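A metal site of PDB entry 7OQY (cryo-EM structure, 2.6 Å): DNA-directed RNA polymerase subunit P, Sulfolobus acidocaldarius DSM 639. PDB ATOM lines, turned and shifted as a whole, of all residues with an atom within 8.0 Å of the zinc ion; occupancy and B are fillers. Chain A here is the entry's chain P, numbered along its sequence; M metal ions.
Of the 20 residues printed, 4 come within 4 Å of the zinc ion.
OE2 of Glu 12 is bound to the zinc ion, 2.0 Å away.
The zinc ion is bound by SG of Cys 6, 2.3 Å away.
The zinc ion is bound by SG of Cys 29 (2.3 Å).
The side-chain sulfur (SG) of Cys 26 binds the zinc ion (2.3 Å).
The side-chain sulfur (SG) of Cys 26 sits close to the backbone NH (N) of Tyr 28.
SG of Cys 29 lies close to N of Tyr 31, at 3.7 Å.
The backbone NH of Cys 6 is in hydrogen-bond range of the backbone carbonyl oxygen of Leu 13, at 3.4 Å.
The backbone NH (N) of Cys 6 sits at hydrogen-bond distance from the side-chain carboxylate (OD1) of Asp 15 (3.5 Å).
O of Tyr 31 lies within hydrogen-bond range of N of Cys 26, at 2.7 Å.
The side-chain carboxylate (OE1) of Glu 12 is in hydrogen-bond range of the backbone NH (N) of Lys 8 (3.1 Å).
The guanidinium group of Arg 5 is in hydrogen-bond range of the backbone carbonyl oxygen of Glu 12 (3.2 Å).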
ATOM      1  N   ARG A   5      -2.171   3.963   0.728  1.00  0.00           N
ATOM      2  CA  ARG A   5      -1.161   2.913   0.678  1.00  0.00           C
ATOM      3  C   ARG A   5      -0.628   2.832  -0.742  1.00  0.00           C
ATOM      4  O   ARG A   5      -1.392   2.589  -1.681  1.00  0.00           O
ATOM      5  CB  ARG A   5      -1.739   1.561   1.108  1.00  0.00           C
ATOM      6  CG  ARG A   5      -0.718   0.449   1.168  1.00  0.00           C
ATOM      7  CD  ARG A   5      -1.372  -0.921   1.034  1.00  0.00           C
ATOM      8  NE  ARG A   5      -2.164  -1.277   2.207  1.00  0.00           N
ATOM      9  CZ  ARG A   5      -1.669  -1.613   3.385  1.00  0.00           C
ATOM     10  NH1 ARG A   5      -0.357  -1.653   3.594  1.00  0.00           N
ATOM     11  NH2 ARG A   5      -2.495  -1.922   4.381  1.00  0.00           N
ATOM     12  N   CYS A   6       0.685   3.043  -0.889  1.00  0.00           N
ATOM     13  CA  CYS A   6       1.300   2.917  -2.204  1.00  0.00           C
ATOM     14  C   CYS A   6       1.198   1.473  -2.676  1.00  0.00           C
ATOM     15  O   CYS A   6       1.663   0.559  -2.011  1.00  0.00           O
ATOM     16  CB  CYS A   6       2.772   3.348  -2.128  1.00  0.00           C
ATOM     17  SG  CYS A   6       3.710   3.081  -3.649  1.00  0.00           S
ATOM     18  N   GLY A   7       0.560   1.273  -3.826  1.00  0.00           N
ATOM     19  CA  GLY A   7       0.365  -0.084  -4.276  1.00  0.00           C
ATOM     20  C   GLY A   7       1.350  -0.570  -5.324  1.00  0.00           C
ATOM     21  O   GLY A   7       1.159  -0.328  -6.517  1.00  0.00           O
ATOM     22  N   LYS A   8       2.379  -1.282  -4.884  1.00  0.00           N
ATOM     23  CA  LYS A   8       3.204  -2.125  -5.755  1.00  0.00           C
ATOM     24  C   LYS A   8       2.796  -3.583  -5.674  1.00  0.00           C
ATOM     25  O   LYS A   8       3.039  -4.345  -6.608  1.00  0.00           O
ATOM     26  CB  LYS A   8       4.684  -1.986  -5.395  1.00  0.00           C
ATOM     27  CG  LYS A   8       5.322  -0.685  -5.864  1.00  0.00           C
ATOM     28  CD  LYS A   8       5.464  -0.650  -7.379  1.00  0.00           C
ATOM     29  CE  LYS A   8       6.664  -1.464  -7.838  1.00  0.00           C
ATOM     30  NZ  LYS A   8       6.611  -1.737  -9.300  1.00  0.00           N
ATOM     31  N   CYS A   9       2.184  -3.963  -4.558  1.00  0.00           N
ATOM     32  CA  CYS A   9       1.579  -5.269  -4.347  1.00  0.00           C
ATOM     33  C   CYS A   9       0.369  -5.041  -3.441  1.00  0.00           C
ATOM     34  O   CYS A   9      -0.151  -3.925  -3.361  1.00  0.00           O
ATOM     35  CB  CYS A   9       2.598  -6.255  -3.761  1.00  0.00           C
ATOM     36  SG  CYS A   9       2.061  -7.988  -3.800  1.00  0.00           S
ATOM     37  N   LYS A  11       0.328  -4.953  -0.259  1.00  0.00           N
ATOM     38  CA  LYS A  11       0.707  -4.093   0.857  1.00  0.00           C
ATOM     39  C   LYS A  11       2.083  -3.484   0.611  1.00  0.00           C
ATOM     40  O   LYS A  11       3.002  -4.174   0.165  1.00  0.00           O
ATOM     41  CB  LYS A  11       0.712  -4.859   2.179  1.00  0.00           C
ATOM     42  CG  LYS A  11      -0.565  -5.648   2.448  1.00  0.00           C
ATOM     43  CD  LYS A  11      -0.493  -6.384   3.766  1.00  0.00           C
ATOM     44  CE  LYS A  11      -0.670  -5.435   4.945  1.00  0.00           C
ATOM     45  NZ  LYS A  11      -1.034  -6.161   6.187  1.00  0.00           N
ATOM     46  N   GLU A  12       2.214  -2.189   0.905  1.00  0.00           N
ATOM     47  CA  GLU A  12       3.480  -1.473   0.907  1.00  0.00           C
ATOM     48  C   GLU A  12       3.387  -0.418   1.998  1.00  0.00           C
ATOM     49  O   GLU A  12       2.453  -0.419   2.811  1.00  0.00           O
ATOM     50  CB  GLU A  12       3.783  -0.912  -0.491  1.00  0.00           C
ATOM     51  CG  GLU A  12       5.137  -0.205  -0.676  1.00  0.00           C
ATOM     52  CD  GLU A  12       5.357   0.271  -2.100  1.00  0.00           C
ATOM     53  OE1 GLU A  12       4.448   0.074  -2.934  1.00  0.00           O
ATOM     54  OE2 GLU A  12       6.409   0.898  -2.368  1.00  0.00           O
ATOM     55  N   LEU A  13       4.352   0.503   2.035  1.00  0.00           N
ATOM     56  CA  LEU A  13       4.402   1.530   3.060  1.00  0.00           C
ATOM     57  C   LEU A  13       3.174   2.425   2.995  1.00  0.00           C
ATOM     58  O   LEU A  13       2.676   2.749   1.910  1.00  0.00           O
ATOM     59  CB  LEU A  13       5.672   2.364   2.899  1.00  0.00           C
ATOM     60  CG  LEU A  13       6.994   1.641   3.153  1.00  0.00           C
ATOM     61  CD1 LEU A  13       8.169   2.546   2.824  1.00  0.00           C
ATOM     62  CD2 LEU A  13       7.074   1.164   4.585  1.00  0.00           C
ATOM     63  N   ASP A  14       2.676   2.815   4.168  1.00  0.00           N
ATOM     64  CA  ASP A  14       1.498   3.663   4.267  1.00  0.00           C
ATOM     65  C   ASP A  14       1.890   5.135   4.216  1.00  0.00           C
ATOM     66  O   ASP A  14       2.916   5.538   4.770  1.00  0.00           O
ATOM     67  CB  ASP A  14       0.740   3.366   5.547  1.00  0.00           C
ATOM     68  CG  ASP A  14      -0.090   2.097   5.468  1.00  0.00           C
ATOM     69  OD1 ASP A  14       0.235   1.229   4.639  1.00  0.00           O
ATOM     70  OD2 ASP A  14      -1.064   1.968   6.238  1.00  0.00           O
ATOM     71  N   ASP A  15       1.058   5.937   3.557  1.00  0.00           N
ATOM     72  CA  ASP A  15       1.243   7.372   3.498  1.00  0.00           C
ATOM     73  C   ASP A  15      -0.101   8.060   3.743  1.00  0.00           C
ATOM     74  O   ASP A  15      -1.163   7.482   3.503  1.00  0.00           O
ATOM     75  CB  ASP A  15       1.822   7.829   2.150  1.00  0.00           C
ATOM     76  CG  ASP A  15       1.073   7.276   0.966  1.00  0.00           C
ATOM     77  OD1 ASP A  15       1.301   6.106   0.601  1.00  0.00           O
ATOM     78  OD2 ASP A  15       0.242   8.016   0.392  1.00  0.00           O
ATOM     79  N   ARG A  25       1.550  10.471  -6.195  1.00  0.00           N
ATOM     80  CA  ARG A  25       2.672   9.542  -6.338  1.00  0.00           C
ATOM     81  C   ARG A  25       3.138   9.099  -4.964  1.00  0.00           C
ATOM     82  O   ARG A  25       2.970   9.812  -3.976  1.00  0.00           O
ATOM     83  CB  ARG A  25       3.825  10.187  -7.121  1.00  0.00           C
ATOM     84  CG  ARG A  25       4.517  11.320  -6.388  1.00  0.00           C
ATOM     85  CD  ARG A  25       5.626  11.927  -7.228  1.00  0.00           C
ATOM     86  NE  ARG A  25       5.087  12.580  -8.423  1.00  0.00           N
ATOM     87  CZ  ARG A  25       5.227  12.103  -9.655  1.00  0.00           C
ATOM     88  NH1 ARG A  25       5.884  10.984  -9.905  1.00  0.00           N
ATOM     89  NH2 ARG A  25       4.695  12.781 -10.670  1.00  0.00           N
ATOM     90  N   CYS A  26       3.724   7.915  -4.917  1.00  0.00           N
ATOM     91  CA  CYS A  26       4.275   7.373  -3.675  1.00  0.00           C
ATOM     92  C   CYS A  26       5.546   8.126  -3.323  1.00  0.00           C
ATOM     93  O   CYS A  26       6.485   8.150  -4.132  1.00  0.00           O
ATOM     94  CB  CYS A  26       4.555   5.883  -3.842  1.00  0.00           C
ATOM     95  SG  CYS A  26       5.410   5.073  -2.467  1.00  0.00           S
ATOM     96  N   PRO A  27       5.622   8.778  -2.158  1.00  0.00           N
ATOM     97  CA  PRO A  27       6.852   9.510  -1.813  1.00  0.00           C
ATOM     98  C   PRO A  27       8.082   8.635  -1.726  1.00  0.00           C
ATOM     99  O   PRO A  27       9.177   9.076  -2.085  1.00  0.00           O
ATOM    100  CB  PRO A  27       6.519  10.149  -0.459  1.00  0.00           C
ATOM    101  CG  PRO A  27       5.019  10.108  -0.362  1.00  0.00           C
ATOM    102  CD  PRO A  27       4.601   8.884  -1.097  1.00  0.00           C
ATOM    103  N   TYR A  28       7.937   7.396  -1.252  1.00  0.00           N
ATOM    104  CA  TYR A  28       9.087   6.530  -1.019  1.00  0.00           C
ATOM    105  C   TYR A  28       9.648   5.957  -2.314  1.00  0.00           C
ATOM    106  O   TYR A  28      10.867   5.815  -2.454  1.00  0.00           O
ATOM    107  CB  TYR A  28       8.710   5.419  -0.048  1.00  0.00           C
ATOM    108  CG  TYR A  28       7.927   5.901   1.155  1.00  0.00           C
ATOM    109  CD1 TYR A  28       8.475   6.820   2.041  1.00  0.00           C
ATOM    110  CD2 TYR A  28       6.641   5.441   1.393  1.00  0.00           C
ATOM    111  CE1 TYR A  28       7.767   7.263   3.138  1.00  0.00           C
ATOM    112  CE2 TYR A  28       5.919   5.887   2.488  1.00  0.00           C
ATOM    113  CZ  TYR A  28       6.483   6.800   3.352  1.00  0.00           C
ATOM    114  OH  TYR A  28       5.774   7.236   4.441  1.00  0.00           O
ATOM    115  N   CYS A  29       8.780   5.608  -3.269  1.00  0.00           N
ATOM    116  CA  CYS A  29       9.216   4.934  -4.488  1.00  0.00           C
ATOM    117  C   CYS A  29       8.796   5.621  -5.778  1.00  0.00           C
ATOM    118  O   CYS A  29       9.256   5.206  -6.844  1.00  0.00           O
ATOM    119  CB  CYS A  29       8.716   3.488  -4.509  1.00  0.00           C
ATOM    120  SG  CYS A  29       6.911   3.312  -4.553  1.00  0.00           S
ATOM    121  N   GLY A  30       7.938   6.631  -5.728  1.00  0.00           N
ATOM    122  CA  GLY A  30       7.565   7.360  -6.923  1.00  0.00           C
ATOM    123  C   GLY A  30       6.496   6.716  -7.770  1.00  0.00           C
ATOM    124  O   GLY A  30       6.201   7.232  -8.856  1.00  0.00           O
ATOM    125  N   TYR A  31       5.902   5.604  -7.329  1.00  0.00           N
ATOM    126  CA  TYR A  31       4.881   4.947  -8.127  1.00  0.00           C
ATOM    127  C   TYR A  31       3.630   5.813  -8.189  1.00  0.00           C
ATOM    128  O   TYR A  31       3.354   6.598  -7.288  1.00  0.00           O
ATOM    129  CB  TYR A  31       4.554   3.577  -7.546  1.00  0.00           C
ATOM    130  CG  TYR A  31       3.823   2.674  -8.503  1.00  0.00           C
ATOM    131  CD1 TYR A  31       4.091   2.725  -9.864  1.00  0.00           C
ATOM    132  CD2 TYR A  31       2.875   1.770  -8.067  1.00  0.00           C
ATOM    133  CE1 TYR A  31       3.435   1.905 -10.754  1.00  0.00           C
ATOM    134  CE2 TYR A  31       2.207   0.937  -8.944  1.00  0.00           C
ATOM    135  CZ  TYR A  31       2.494   1.015 -10.290  1.00  0.00           C
ATOM    136  OH  TYR A  31       1.826   0.183 -11.167  1.00  0.00           O
ATOM    137  N   ARG A  32       2.857   5.651  -9.270  1.00  0.00           N
ATOM    138  CA  ARG A  32       1.799   6.582  -9.611  1.00  0.00           C
ATOM    139  C   ARG A  32       0.399   6.081  -9.272  1.00  0.00           C
ATOM    140  O   ARG A  32      -0.583   6.714  -9.670  1.00  0.00           O
ATOM    141  CB  ARG A  32       1.863   6.911 -11.107  1.00  0.00           C
ATOM    142  CG  ARG A  32       3.237   7.367 -11.579  1.00  0.00           C
ATOM    143  CD  ARG A  32       3.447   8.841 -11.320  1.00  0.00           C
ATOM    144  NE  ARG A  32       2.359   9.642 -11.852  1.00  0.00           N
ATOM    145  CZ  ARG A  32       2.506  10.648 -12.697  1.00  0.00           C
ATOM    146  NH1 ARG A  32       3.703  10.998 -13.141  1.00  0.00           N
ATOM    147  NH2 ARG A  32       1.433  11.314 -13.119  1.00  0.00           N
ATOM    148  N   ILE A  33       0.275   4.976  -8.542  1.00  0.00           N
ATOM    149  CA  ILE A  33      -1.019   4.436  -8.147  1.00  0.00           C
ATOM    150  C   ILE A  33      -1.010   4.196  -6.644  1.00  0.00           C
ATOM    151  O   ILE A  33      -0.138   3.492  -6.132  1.00  0.00           O
ATOM    152  CB  ILE A  33      -1.363   3.141  -8.904  1.00  0.00           C
ATOM    153  CG1 ILE A  33      -1.377   3.387 -10.412  1.00  0.00           C
ATOM    154  CG2 ILE A  33      -2.703   2.608  -8.444  1.00  0.00           C
ATOM    155  CD1 ILE A  33      -0.909   2.213 -11.226  1.00  0.00           C
ATOM    156  N   ILE A  34      -1.981   4.787  -5.939  1.00  0.00           N
ATOM    157  CA  ILE A  34      -2.132   4.600  -4.501  1.00  0.00           C
ATOM    158  C   ILE A  34      -3.572   4.182  -4.209  1.00  0.00           C
ATOM    159  O   ILE A  34      -4.486   4.418  -4.994  1.00  0.00           O
ATOM    160  CB  ILE A  34      -1.763   5.875  -3.700  1.00  0.00           C
ATOM    161  CG1 ILE A  34      -2.792   6.984  -3.948  1.00  0.00           C
ATOM    162  CG2 ILE A  34      -0.373   6.353  -4.057  1.00  0.00           C
ATOM    163  CD1 ILE A  34      -2.409   8.310  -3.345  1.00  0.00           C
HETATM  164 ZN    ZN M   1       5.754   2.796  -2.634  1.00  0.00          ZN
